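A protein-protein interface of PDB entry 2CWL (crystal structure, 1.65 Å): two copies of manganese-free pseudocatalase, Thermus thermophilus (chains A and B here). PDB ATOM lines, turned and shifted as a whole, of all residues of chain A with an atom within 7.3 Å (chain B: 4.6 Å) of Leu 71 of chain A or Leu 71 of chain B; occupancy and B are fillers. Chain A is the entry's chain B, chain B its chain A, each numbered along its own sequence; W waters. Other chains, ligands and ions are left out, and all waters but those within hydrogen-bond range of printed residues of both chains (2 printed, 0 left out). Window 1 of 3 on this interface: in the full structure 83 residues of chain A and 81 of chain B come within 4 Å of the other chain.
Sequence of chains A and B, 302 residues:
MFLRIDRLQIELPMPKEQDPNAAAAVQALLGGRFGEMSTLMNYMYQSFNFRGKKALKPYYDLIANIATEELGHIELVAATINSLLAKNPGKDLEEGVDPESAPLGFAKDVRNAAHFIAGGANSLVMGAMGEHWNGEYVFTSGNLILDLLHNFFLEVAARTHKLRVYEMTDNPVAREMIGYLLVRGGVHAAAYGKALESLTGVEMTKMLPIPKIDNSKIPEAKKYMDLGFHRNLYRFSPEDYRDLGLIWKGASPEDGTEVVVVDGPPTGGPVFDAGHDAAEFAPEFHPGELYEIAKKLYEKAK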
ATOM      1  N   MET A   1     -33.439  -9.215 -31.605  1.00  0.00           N
ATOM      2  CA  MET A   1     -32.283  -8.469 -31.025  1.00  0.00           C
ATOM      3  C   MET A   1     -32.444  -8.327 -29.517  1.00  0.00           C
ATOM      4  O   MET A   1     -33.532  -8.537 -28.973  1.00  0.00           O
ATOM      5  CB  MET A   1     -32.171  -7.075 -31.650  1.00  0.00           C
ATOM      6  CG  MET A   1     -31.868  -7.071 -33.136  1.00  0.00           C
ATOM      7  SD  MET A   1     -31.643  -5.384 -33.737  1.00  0.00           S
ATOM      8  CE  MET A   1     -33.335  -4.946 -34.154  1.00  0.00           C
ATOM      9  N   PHE A   2     -31.359  -7.961 -28.845  1.00  0.00           N
ATOM     10  CA  PHE A   2     -31.387  -7.807 -27.395  1.00  0.00           C
ATOM     11  C   PHE A   2     -30.689  -6.546 -26.900  1.00  0.00           C
ATOM     12  O   PHE A   2     -29.842  -5.971 -27.592  1.00  0.00           O
ATOM     13  CB  PHE A   2     -30.743  -9.028 -26.724  1.00  0.00           C
ATOM     14  CG  PHE A   2     -31.459 -10.320 -26.999  1.00  0.00           C
ATOM     15  CD1 PHE A   2     -31.319 -10.964 -28.226  1.00  0.00           C
ATOM     16  CD2 PHE A   2     -32.305 -10.872 -26.046  1.00  0.00           C
ATOM     17  CE1 PHE A   2     -32.019 -12.139 -28.498  1.00  0.00           C
ATOM     18  CE2 PHE A   2     -33.011 -12.048 -26.307  1.00  0.00           C
ATOM     19  CZ  PHE A   2     -32.868 -12.681 -27.535  1.00  0.00           C
ATOM     20  N   LEU A   3     -31.069  -6.121 -25.699  1.00  0.00           N
ATOM     21  CA  LEU A   3     -30.482  -4.962 -25.042  1.00  0.00           C
ATOM     22  C   LEU A   3     -29.994  -5.452 -23.685  1.00  0.00           C
ATOM     23  O   LEU A   3     -30.443  -6.491 -23.194  1.00  0.00           O
ATOM     24  CB  LEU A   3     -31.523  -3.858 -24.834  1.00  0.00           C
ATOM     25  CG  LEU A   3     -32.232  -3.304 -26.070  1.00  0.00           C
ATOM     26  CD1 LEU A   3     -33.259  -2.273 -25.624  1.00  0.00           C
ATOM     27  CD2 LEU A   3     -31.227  -2.680 -27.026  1.00  0.00           C
ATOM     28  N   ARG A   4     -29.089  -4.701 -23.075  1.00  0.00           N
ATOM     29  CA  ARG A   4     -28.548  -5.082 -21.781  1.00  0.00           C
ATOM     30  C   ARG A   4     -28.631  -3.944 -20.767  1.00  0.00           C
ATOM     31  O   ARG A   4     -28.461  -2.775 -21.114  1.00  0.00           O
ATOM     32  CB  ARG A   4     -27.089  -5.518 -21.949  1.00  0.00           C
ATOM     33  CG  ARG A   4     -26.415  -6.001 -20.672  1.00  0.00           C
ATOM     34  CD  ARG A   4     -25.030  -6.566 -20.972  1.00  0.00           C
ATOM     35  NE  ARG A   4     -24.436  -7.182 -19.787  1.00  0.00           N
ATOM     36  CZ  ARG A   4     -23.436  -8.057 -19.826  1.00  0.00           C
ATOM     37  NH1 ARG A   4     -22.913  -8.418 -20.991  1.00  0.00           N
ATOM     38  NH2 ARG A   4     -22.971  -8.586 -18.701  1.00  0.00           N
ATOM     39  N   GLN A   9     -30.135  -9.303 -11.451  1.00  0.00           N
ATOM     40  CA  GLN A   9     -31.580  -9.311 -11.248  1.00  0.00           C
ATOM     41  C   GLN A   9     -31.965  -8.974  -9.815  1.00  0.00           C
ATOM     42  O   GLN A   9     -33.080  -8.520  -9.554  1.00  0.00           O
ATOM     43  CB  GLN A   9     -32.187 -10.651 -11.657  1.00  0.00           C
ATOM     44  CG  GLN A   9     -33.668 -10.515 -11.960  1.00  0.00           C
ATOM     45  CD  GLN A   9     -34.245 -11.722 -12.660  1.00  0.00           C
ATOM     46  OE1 GLN A   9     -33.611 -12.303 -13.539  1.00  0.00           O
ATOM     47  NE2 GLN A   9     -35.465 -12.091 -12.292  1.00  0.00           N
ATOM     48  N   GLU A  36     -28.821 -23.002 -15.164  1.00  0.00           N
ATOM     49  CA  GLU A  36     -29.465 -21.898 -15.861  1.00  0.00           C
ATOM     50  C   GLU A  36     -29.063 -21.793 -17.334  1.00  0.00           C
ATOM     51  O   GLU A  36     -29.791 -21.206 -18.135  1.00  0.00           O
ATOM     52  CB  GLU A  36     -29.189 -20.583 -15.124  1.00  0.00           C
ATOM     53  CG  GLU A  36     -29.731 -20.546 -13.690  1.00  0.00           C
ATOM     54  CD  GLU A  36     -31.251 -20.602 -13.609  1.00  0.00           C
ATOM     55  OE1 GLU A  36     -31.917 -20.559 -14.663  1.00  0.00           O
ATOM     56  OE2 GLU A  36     -31.783 -20.684 -12.479  1.00  0.00           O
ATOM     57  N   THR A  39     -31.828 -23.878 -19.060  1.00  0.00           N
ATOM     58  CA  THR A  39     -33.132 -23.245 -19.163  1.00  0.00           C
ATOM     59  C   THR A  39     -32.995 -22.116 -20.187  1.00  0.00           C
ATOM     60  O   THR A  39     -33.866 -21.919 -21.034  1.00  0.00           O
ATOM     61  CB  THR A  39     -33.612 -22.711 -17.793  1.00  0.00           C
ATOM     62  OG1 THR A  39     -32.510 -22.138 -17.077  1.00  0.00           O
ATOM     63  CG2 THR A  39     -34.204 -23.850 -16.966  1.00  0.00           C
ATOM     64  N   LEU A  40     -31.880 -21.395 -20.134  1.00  0.00           N
ATOM     65  CA  LEU A  40     -31.648 -20.311 -21.085  1.00  0.00           C
ATOM     66  C   LEU A  40     -31.644 -20.780 -22.538  1.00  0.00           C
ATOM     67  O   LEU A  40     -32.446 -20.321 -23.354  1.00  0.00           O
ATOM     68  CB  LEU A  40     -30.310 -19.618 -20.799  1.00  0.00           C
ATOM     69  CG  LEU A  40     -29.789 -18.733 -21.940  1.00  0.00           C
ATOM     70  CD1 LEU A  40     -30.764 -17.584 -22.195  1.00  0.00           C
ATOM     71  CD2 LEU A  40     -28.410 -18.201 -21.590  1.00  0.00           C
ATOM     72  N   MET A  41     -30.734 -21.692 -22.867  1.00  0.00           N
ATOM     73  CA  MET A  41     -30.623 -22.152 -24.244  1.00  0.00           C
ATOM     74  C   MET A  41     -31.815 -22.944 -24.767  1.00  0.00           C
ATOM     75  O   MET A  41     -32.105 -22.913 -25.964  1.00  0.00           O
ATOM     76  CB  MET A  41     -29.319 -22.931 -24.427  1.00  0.00           C
ATOM     77  CG  MET A  41     -28.074 -22.048 -24.307  1.00  0.00           C
ATOM     78  SD  MET A  41     -27.978 -20.758 -25.587  1.00  0.00           S
ATOM     79  CE  MET A  41     -26.713 -19.690 -24.905  1.00  0.00           C
ATOM     80  N   MET A  44     -34.374 -20.191 -25.486  1.00  0.00           N
ATOM     81  CA  MET A  44     -33.852 -19.318 -26.529  1.00  0.00           C
ATOM     82  C   MET A  44     -34.004 -19.974 -27.904  1.00  0.00           C
ATOM     83  O   MET A  44     -34.555 -19.372 -28.827  1.00  0.00           O
ATOM     84  CB  MET A  44     -32.381 -18.986 -26.257  1.00  0.00           C
ATOM     85  CG  MET A  44     -31.814 -17.901 -27.167  1.00  0.00           C
ATOM     86  SD  MET A  44     -32.694 -16.316 -27.032  1.00  0.00           S
ATOM     87  CE  MET A  44     -32.025 -15.690 -25.500  1.00  0.00           C
ATOM     88  N   PHE A  48     -36.441 -19.193 -31.197  1.00  0.00           N
ATOM     89  CA  PHE A  48     -35.971 -18.970 -32.563  1.00  0.00           C
ATOM     90  C   PHE A  48     -36.730 -19.884 -33.522  1.00  0.00           C
ATOM     91  O   PHE A  48     -37.212 -19.454 -34.573  1.00  0.00           O
ATOM     92  CB  PHE A  48     -34.478 -19.305 -32.718  1.00  0.00           C
ATOM     93  CG  PHE A  48     -33.549 -18.454 -31.895  1.00  0.00           C
ATOM     94  CD1 PHE A  48     -33.923 -17.189 -31.449  1.00  0.00           C
ATOM     95  CD2 PHE A  48     -32.260 -18.910 -31.615  1.00  0.00           C
ATOM     96  CE1 PHE A  48     -33.029 -16.389 -30.739  1.00  0.00           C
ATOM     97  CE2 PHE A  48     -31.358 -18.116 -30.905  1.00  0.00           C
ATOM     98  CZ  PHE A  48     -31.741 -16.855 -30.467  1.00  0.00           C
ATOM     99  N   ASN A  65     -40.127 -14.534 -24.036  1.00  0.00           N
ATOM    100  CA  ASN A  65     -39.900 -13.689 -22.872  1.00  0.00           C
ATOM    101  C   ASN A  65     -39.124 -14.380 -21.759  1.00  0.00           C
ATOM    102  O   ASN A  65     -38.173 -13.817 -21.216  1.00  0.00           O
ATOM    103  CB  ASN A  65     -41.227 -13.183 -22.309  1.00  0.00           C
ATOM    104  CG  ASN A  65     -41.029 -12.218 -21.159  1.00  0.00           C
ATOM    105  OD1 ASN A  65     -40.483 -11.128 -21.336  1.00  0.00           O
ATOM    106  ND2 ASN A  65     -41.461 -12.618 -19.969  1.00  0.00           N
ATOM    107  N   ILE A  66     -39.529 -15.595 -21.407  1.00  0.00           N
ATOM    108  CA  ILE A  66     -38.835 -16.304 -20.345  1.00  0.00           C
ATOM    109  C   ILE A  66     -37.384 -16.561 -20.750  1.00  0.00           C
ATOM    110  O   ILE A  66     -36.486 -16.502 -19.911  1.00  0.00           O
ATOM    111  CB  ILE A  66     -39.566 -17.615 -19.984  1.00  0.00           C
ATOM    112  CG1 ILE A  66     -40.938 -17.270 -19.383  1.00  0.00           C
ATOM    113  CG2 ILE A  66     -38.745 -18.420 -18.983  1.00  0.00           C
ATOM    114  CD1 ILE A  66     -41.787 -18.469 -18.996  1.00  0.00           C
ATOM    115  N   ALA A  67     -37.151 -16.819 -22.034  1.00  0.00           N
ATOM    116  CA  ALA A  67     -35.791 -17.042 -22.520  1.00  0.00           C
ATOM    117  C   ALA A  67     -34.944 -15.814 -22.186  1.00  0.00           C
ATOM    118  O   ALA A  67     -33.768 -15.926 -21.844  1.00  0.00           O
ATOM    119  CB  ALA A  67     -35.798 -17.271 -24.029  1.00  0.00           C
ATOM    120  N   THR A  68     -35.555 -14.636 -22.289  1.00  0.00           N
ATOM    121  CA  THR A  68     -34.856 -13.393 -21.996  1.00  0.00           C
ATOM    122  C   THR A  68     -34.543 -13.283 -20.505  1.00  0.00           C
ATOM    123  O   THR A  68     -33.467 -12.820 -20.128  1.00  0.00           O
ATOM    124  CB  THR A  68     -35.683 -12.175 -22.456  1.00  0.00           C
ATOM    125  OG1 THR A  68     -36.053 -12.357 -23.828  1.00  0.00           O
ATOM    126  CG2 THR A  68     -34.865 -10.887 -22.330  1.00  0.00           C
ATOM    127  N   GLU A  69     -35.468 -13.709 -19.650  1.00  0.00           N
ATOM    128  CA  GLU A  69     -35.190 -13.648 -18.221  1.00  0.00           C
ATOM    129  C   GLU A  69     -34.029 -14.578 -17.884  1.00  0.00           C
ATOM    130  O   GLU A  69     -33.211 -14.271 -17.020  1.00  0.00           O
ATOM    131  CB  GLU A  69     -36.403 -14.050 -17.372  1.00  0.00           C
ATOM    132  CG  GLU A  69     -36.096 -13.875 -15.879  1.00  0.00           C
ATOM    133  CD  GLU A  69     -37.233 -14.225 -14.934  1.00  0.00           C
ATOM    134  OE1 GLU A  69     -38.392 -14.371 -15.376  1.00  0.00           O
ATOM    135  OE2 GLU A  69     -36.950 -14.337 -13.723  1.00  0.00           O
ATOM    136  N   GLU A  70     -33.961 -15.719 -18.567  1.00  0.00           N
ATOM    137  CA  GLU A  70     -32.896 -16.686 -18.307  1.00  0.00           C
ATOM    138  C   GLU A  70     -31.501 -16.094 -18.499  1.00  0.00           C
ATOM    139  O   GLU A  70     -30.542 -16.548 -17.877  1.00  0.00           O
ATOM    140  CB  GLU A  70     -33.054 -17.917 -19.202  1.00  0.00           C
ATOM    141  CG  GLU A  70     -34.342 -18.717 -18.993  1.00  0.00           C
ATOM    142  CD  GLU A  70     -34.440 -19.360 -17.619  1.00  0.00           C
ATOM    143  OE1 GLU A  70     -33.391 -19.601 -16.986  1.00  0.00           O
ATOM    144  OE2 GLU A  70     -35.577 -19.641 -17.184  1.00  0.00           O
ATOM    145  N   LEU A  71     -31.380 -15.092 -19.364  1.00  0.00           N
ATOM    146  CA  LEU A  71     -30.082 -14.456 -19.585  1.00  0.00           C
ATOM    147  C   LEU A  71     -29.629 -13.841 -18.266  1.00  0.00           C
ATOM    148  O   LEU A  71     -28.446 -13.869 -17.924  1.00  0.00           O
ATOM    149  CB  LEU A  71     -30.191 -13.370 -20.660  1.00  0.00           C
ATOM    150  CG  LEU A  71     -30.401 -13.879 -22.091  1.00  0.00           C
ATOM    151  CD1 LEU A  71     -30.825 -12.731 -23.003  1.00  0.00           C
ATOM    152  CD2 LEU A  71     -29.110 -14.520 -22.590  1.00  0.00           C
ATOM    153  N   GLY A  72     -30.589 -13.292 -17.525  1.00  0.00           N
ATOM    154  CA  GLY A  72     -30.282 -12.693 -16.239  1.00  0.00           C
ATOM    155  C   GLY A  72     -29.991 -13.765 -15.206  1.00  0.00           C
ATOM    156  O   GLY A  72     -29.279 -13.525 -14.227  1.00  0.00           O
ATOM    157  N   HIS A  73     -30.543 -14.954 -15.419  1.00  0.00           N
ATOM    158  CA  HIS A  73     -30.311 -16.054 -14.496  1.00  0.00           C
ATOM    159  C   HIS A  73     -28.878 -16.569 -14.590  1.00  0.00           C
ATOM    160  O   HIS A  73     -28.250 -16.805 -13.562  1.00  0.00           O
ATOM    161  CB  HIS A  73     -31.309 -17.191 -14.739  1.00  0.00           C
ATOM    162  CG  HIS A  73     -32.701 -16.876 -14.285  1.00  0.00           C
ATOM    163  ND1 HIS A  73     -33.699 -17.824 -14.230  1.00  0.00           N
ATOM    164  CD2 HIS A  73     -33.257 -15.720 -13.847  1.00  0.00           C
ATOM    165  CE1 HIS A  73     -34.808 -17.269 -13.775  1.00  0.00           C
ATOM    166  NE2 HIS A  73     -34.567 -15.992 -13.533  1.00  0.00           N
ATOM    167  N   ILE A  74     -28.343 -16.750 -15.798  1.00  0.00           N
ATOM    168  CA  ILE A  74     -26.964 -17.225 -15.876  1.00  0.00           C
ATOM    169  C   ILE A  74     -26.048 -16.137 -15.332  1.00  0.00           C
ATOM    170  O   ILE A  74     -25.029 -16.426 -14.705  1.00  0.00           O
ATOM    171  CB  ILE A  74     -26.516 -17.624 -17.321  1.00  0.00           C
ATOM    172  CG1 ILE A  74     -26.593 -16.432 -18.277  1.00  0.00           C
ATOM    173  CG2 ILE A  74     -27.362 -18.797 -17.812  1.00  0.00           C
ATOM    174  CD1 ILE A  74     -25.849 -16.675 -19.592  1.00  0.00           C
ATOM    175  N   GLU A  75     -26.427 -14.881 -15.555  1.00  0.00           N
ATOM    176  CA  GLU A  75     -25.637 -13.759 -15.061  1.00  0.00           C
ATOM    177  C   GLU A  75     -25.599 -13.773 -13.532  1.00  0.00           C
ATOM    178  O   GLU A  75     -24.549 -13.551 -12.927  1.00  0.00           O
ATOM    179  CB  GLU A  75     -26.230 -12.433 -15.557  1.00  0.00           C
ATOM    180  CG  GLU A  75     -25.577 -11.193 -14.955  1.00  0.00           C
ATOM    181  CD  GLU A  75     -26.164  -9.896 -15.489  1.00  0.00           C
ATOM    182  OE1 GLU A  75     -27.368  -9.879 -15.821  1.00  0.00           O
ATOM    183  OE2 GLU A  75     -25.425  -8.889 -15.560  1.00  0.00           O
ATOM    184  N   LEU A  76     -26.743 -14.040 -12.909  1.00  0.00           N
ATOM    185  CA  LEU A  76     -26.825 -14.062 -11.452  1.00  0.00           C
ATOM    186  C   LEU A  76     -26.048 -15.225 -10.830  1.00  0.00           C
ATOM    187  O   LEU A  76     -25.373 -15.052  -9.813  1.00  0.00           O
ATOM    188  CB  LEU A  76     -28.289 -14.113 -11.007  1.00  0.00           C
ATOM    189  CG  LEU A  76     -28.514 -13.960  -9.498  1.00  0.00           C
ATOM    190  CD1 LEU A  76     -28.057 -12.579  -9.043  1.00  0.00           C
ATOM    191  CD2 LEU A  76     -29.984 -14.162  -9.177  1.00  0.00           C
ATOM    192  N   PHE B   2     -31.205  -8.445 -19.189  1.00  0.00           N
ATOM    193  CA  PHE B   2     -31.370  -8.211 -20.617  1.00  0.00           C
ATOM    194  C   PHE B   2     -32.817  -7.989 -21.022  1.00  0.00           C
ATOM    195  O   PHE B   2     -33.747  -8.371 -20.305  1.00  0.00           O
ATOM    196  CB  PHE B   2     -30.806  -9.394 -21.411  1.00  0.00           C
ATOM    197  CG  PHE B   2     -29.341  -9.621 -21.196  1.00  0.00           C
ATOM    198  CD1 PHE B   2     -28.880 -10.244 -20.037  1.00  0.00           C
ATOM    199  CD2 PHE B   2     -28.415  -9.166 -22.124  1.00  0.00           C
ATOM    200  CE1 PHE B   2     -27.517 -10.403 -19.809  1.00  0.00           C
ATOM    201  CE2 PHE B   2     -27.047  -9.320 -21.905  1.00  0.00           C
ATOM    202  CZ  PHE B   2     -26.598  -9.938 -20.745  1.00  0.00           C
ATOM    203  N   LEU B  40     -20.555 -15.152 -28.776  1.00  0.00           N
ATOM    204  CA  LEU B  40     -21.526 -14.778 -27.749  1.00  0.00           C
ATOM    205  C   LEU B  40     -21.103 -15.192 -26.342  1.00  0.00           C
ATOM    206  O   LEU B  40     -20.975 -14.356 -25.449  1.00  0.00           O
ATOM    207  CB  LEU B  40     -22.895 -15.404 -28.042  1.00  0.00           C
ATOM    208  CG  LEU B  40     -23.882 -15.396 -26.861  1.00  0.00           C
ATOM    209  CD1 LEU B  40     -24.236 -13.964 -26.482  1.00  0.00           C
ATOM    210  CD2 LEU B  40     -25.137 -16.171 -27.230  1.00  0.00           C
ATOM    211  N   MET B  44     -19.836 -12.927 -23.247  1.00  0.00           N
ATOM    212  CA  MET B  44     -20.815 -12.926 -22.168  1.00  0.00           C
ATOM    213  C   MET B  44     -20.145 -13.299 -20.849  1.00  0.00           C
ATOM    214  O   MET B  44     -20.274 -12.583 -19.854  1.00  0.00           O
ATOM    215  CB  MET B  44     -21.956 -13.900 -22.477  1.00  0.00           C
ATOM    216  CG  MET B  44     -23.141 -13.814 -21.516  1.00  0.00           C
ATOM    217  SD  MET B  44     -23.926 -12.173 -21.478  1.00  0.00           S
ATOM    218  CE  MET B  44     -24.832 -12.197 -23.010  1.00  0.00           C
ATOM    219  N   ALA B  67     -21.052  -8.342 -26.316  1.00  0.00           N
ATOM    220  CA  ALA B  67     -21.661  -9.606 -25.913  1.00  0.00           C
ATOM    221  C   ALA B  67     -23.166  -9.536 -26.173  1.00  0.00           C
ATOM    222  O   ALA B  67     -23.786 -10.518 -26.581  1.00  0.00           O
ATOM    223  CB  ALA B  67     -21.397  -9.867 -24.431  1.00  0.00           C
ATOM    224  N   THR B  68     -23.750  -8.364 -25.946  1.00  0.00           N
ATOM    225  CA  THR B  68     -25.177  -8.190 -26.164  1.00  0.00           C
ATOM    226  C   THR B  68     -25.498  -8.283 -27.652  1.00  0.00           C
ATOM    227  O   THR B  68     -26.502  -8.885 -28.037  1.00  0.00           O
ATOM    228  CB  THR B  68     -25.657  -6.836 -25.607  1.00  0.00           C
ATOM    229  OG1 THR B  68     -25.296  -6.744 -24.226  1.00  0.00           O
ATOM    230  CG2 THR B  68     -27.173  -6.709 -25.737  1.00  0.00           C
ATOM    231  N   GLU B  69     -24.652  -7.701 -28.498  1.00  0.00           N
ATOM    232  CA  GLU B  69     -24.912  -7.789 -29.931  1.00  0.00           C
ATOM    233  C   GLU B  69     -24.848  -9.244 -30.387  1.00  0.00           C
ATOM    234  O   GLU B  69     -25.614  -9.658 -31.256  1.00  0.00           O
ATOM    235  CB  GLU B  69     -23.911  -6.971 -30.757  1.00  0.00           C
ATOM    236  CG  GLU B  69     -24.301  -6.970 -32.238  1.00  0.00           C
ATOM    237  CD  GLU B  69     -23.343  -6.221 -33.145  1.00  0.00           C
ATOM    238  OE1 GLU B  69     -22.596  -5.353 -32.657  1.00  0.00           O
ATOM    239  OE2 GLU B  69     -23.363  -6.495 -34.367  1.00  0.00           O
ATOM    240  N   GLU B  70     -23.938 -10.019 -29.798  1.00  0.00           N
ATOM    241  CA  GLU B  70     -23.789 -11.426 -30.164  1.00  0.00           C
ATOM    242  C   GLU B  70     -25.091 -12.214 -30.005  1.00  0.00           C
ATOM    243  O   GLU B  70     -25.296 -13.218 -30.685  1.00  0.00           O
ATOM    244  CB  GLU B  70     -22.685 -12.084 -29.329  1.00  0.00           C
ATOM    245  CG  GLU B  70     -21.283 -11.523 -29.554  1.00  0.00           C
ATOM    246  CD  GLU B  70     -20.797 -11.686 -30.986  1.00  0.00           C
ATOM    247  OE1 GLU B  70     -21.266 -12.613 -31.677  1.00  0.00           O
ATOM    248  OE2 GLU B  70     -19.933 -10.892 -31.415  1.00  0.00           O
ATOM    249  N   LEU B  71     -25.961 -11.774 -29.100  1.00  0.00           N
ATOM    250  CA  LEU B  71     -27.244 -12.449 -28.914  1.00  0.00           C
ATOM    251  C   LEU B  71     -28.042 -12.316 -30.204  1.00  0.00           C
ATOM    252  O   LEU B  71     -28.746 -13.240 -30.614  1.00  0.00           O
ATOM    253  CB  LEU B  71     -28.020 -11.818 -27.755  1.00  0.00           C
ATOM    254  CG  LEU B  71     -27.451 -12.115 -26.363  1.00  0.00           C
ATOM    255  CD1 LEU B  71     -28.074 -11.177 -25.342  1.00  0.00           C
ATOM    256  CD2 LEU B  71     -27.717 -13.574 -26.000  1.00  0.00           C
ATOM    257  N   GLY B  72     -27.929 -11.153 -30.838  1.00  0.00           N
ATOM    258  CA  GLY B  72     -28.626 -10.927 -32.090  1.00  0.00           C
ATOM    259  C   GLY B  72     -27.971 -11.736 -33.193  1.00  0.00           C
ATOM    260  O   GLY B  72     -28.624 -12.131 -34.162  1.00  0.00           O
ATOM    261  N   HIS B  73     -26.676 -11.994 -33.047  1.00  0.00           N
ATOM    262  CA  HIS B  73     -25.965 -12.771 -34.049  1.00  0.00           C
ATOM    263  C   HIS B  73     -26.421 -14.229 -34.048  1.00  0.00           C
ATOM    264  O   HIS B  73     -26.709 -14.771 -35.112  1.00  0.00           O
ATOM    265  CB  HIS B  73     -24.448 -12.682 -33.840  1.00  0.00           C
ATOM    266  CG  HIS B  73     -23.867 -11.345 -34.193  1.00  0.00           C
ATOM    267  ND1 HIS B  73     -22.512 -11.135 -34.329  1.00  0.00           N
ATOM    268  CD2 HIS B  73     -24.458 -10.153 -34.448  1.00  0.00           C
ATOM    269  CE1 HIS B  73     -22.291  -9.875 -34.656  1.00  0.00           C
ATOM    270  NE2 HIS B  73     -23.455  -9.256 -34.734  1.00  0.00           N
ATOM    271  N   ILE B  74     -26.503 -14.875 -32.883  1.00  0.00           N
ATOM    272  CA  ILE B  74     -26.957 -16.265 -32.896  1.00  0.00           C
ATOM    273  C   ILE B  74     -28.398 -16.326 -33.391  1.00  0.00           C
ATOM    274  O   ILE B  74     -28.782 -17.267 -34.081  1.00  0.00           O
ATOM    275  CB  ILE B  74     -26.859 -16.975 -31.503  1.00  0.00           C
ATOM    276  CG1 ILE B  74     -27.731 -16.276 -30.458  1.00  0.00           C
ATOM    277  CG2 ILE B  74     -25.401 -17.046 -31.059  1.00  0.00           C
ATOM    278  CD1 ILE B  74     -27.948 -17.119 -29.202  1.00  0.00           C
ATOM    279  N   GLU B  75     -29.189 -15.311 -33.054  1.00  0.00           N
ATOM    280  CA  GLU B  75     -30.585 -15.264 -33.487  1.00  0.00           C
ATOM    281  C   GLU B  75     -30.666 -15.203 -35.010  1.00  0.00           C
ATOM    282  O   GLU B  75     -31.478 -15.895 -35.627  1.00  0.00           O
ATOM    283  CB  GLU B  75     -31.290 -14.041 -32.882  1.00  0.00           C
ATOM    284  CG  GLU B  75     -32.718 -13.828 -33.384  1.00  0.00           C
ATOM    285  CD  GLU B  75     -33.374 -12.586 -32.797  1.00  0.00           C
ATOM    286  OE1 GLU B  75     -32.645 -11.630 -32.452  1.00  0.00           O
ATOM    287  OE2 GLU B  75     -34.618 -12.561 -32.698  1.00  0.00           O
HETATM  288  O   HOH W   1     -32.861 -10.703 -18.454  1.00  0.00           O
HETATM  289  O   HOH W   2     -28.539  -7.669 -29.568  1.00  0.00           O
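Water W1 lies within hydrogen-bond range of the backbone carbonyl oxygen (O) of Thr 68 of chain A and the backbone NH (N) of Phe 2 of chain B.
Water W2 lies within hydrogen-bond range of O of Thr 68 of chain B and O of Phe 2 of chain A.
Of the printed residues of chain B, Met 1 of chain A touches Glu 75.
Of the printed residues of chain B, Phe 2 of chain A touches Thr 68 and Leu 71.
Printed residues of chain B within 4 Å of Thr 68 of chain A: Phe 2 (3.4 Å).
Leu 71 of chain A touches two residues of chain B.
Of chain A, only Phe 2 (3.4 Å) and Leu 71 (3.8 Å) come within 4 Å of Leu 71 of chain B.
Printed residues of chain A within 4 Å of Ile 74 of chain B: Phe 48.
Phe 2 of chain A touches Thr 68 of chain B, and with the chains exchanged Thr 68 of chain A touches Phe 2 of chain B.
Phe 2 of chain A touches Leu 71 of chain B, and with the chains exchanged Leu 71 of chain A touches Phe 2 of chain B.
Leu 71 of chain B touches its own counterpart, Leu 71 of chain A.
12 positions are printed for both chains.
Of the 13 pairs that touch across the chains among the printed residues, 5 have their exchanged pair printed and touching as well.
NH2 of Arg 4 of chain A is in salt-bridge range of OE2 of Glu 75 of chain A.
O of Phe 2 of chain A touches CG2 of Thr 68 of chain B, 3.3 Å away.
Leu 3 of chain A touches Thr 68 of chain B (C to CG2, 3.7 Å).
Arg 4 of chain A touches Phe 2 of chain B.
SD of Met 44 of chain B touches NH1 of Arg 4 of chain A, 3.9 Å away.
CB of Arg 4 of chain A touches OG1 of Thr 68 of chain B (3.1 Å).
Phe 48 of chain A touches Ile 74 of chain B.
Phe 48 of chain A touches Glu 75 of chain B.
Phe 2 of chain B touches Thr 68 of chain A.
CB of Leu 71 of chain A touches CD1 of Phe 2 of chain B, 3.4 Å away.
CD2 of Leu 71 of chain A touches CD2 of Leu 71 of chain B, at 3.8 Å.
Printed residues of chain A that touch a printed residue of chain B: Met 1, Phe 2, Leu 3, Arg 4, Phe 48, Thr 68 and Leu 71.
Hydrophobic or aromatic side chains of chain A within 4 Å of the printed part of chain B: Phe 2, Phe 48 and Leu 71.
Among the printed residues, no Asp or Glu carboxylate lies within 4 Å of a Lys or Arg side-chain nitrogen of the other chain.
OE1 of Glu 75 of chain B lies within hydrogen-bond range of N of Met 1 of chain A.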
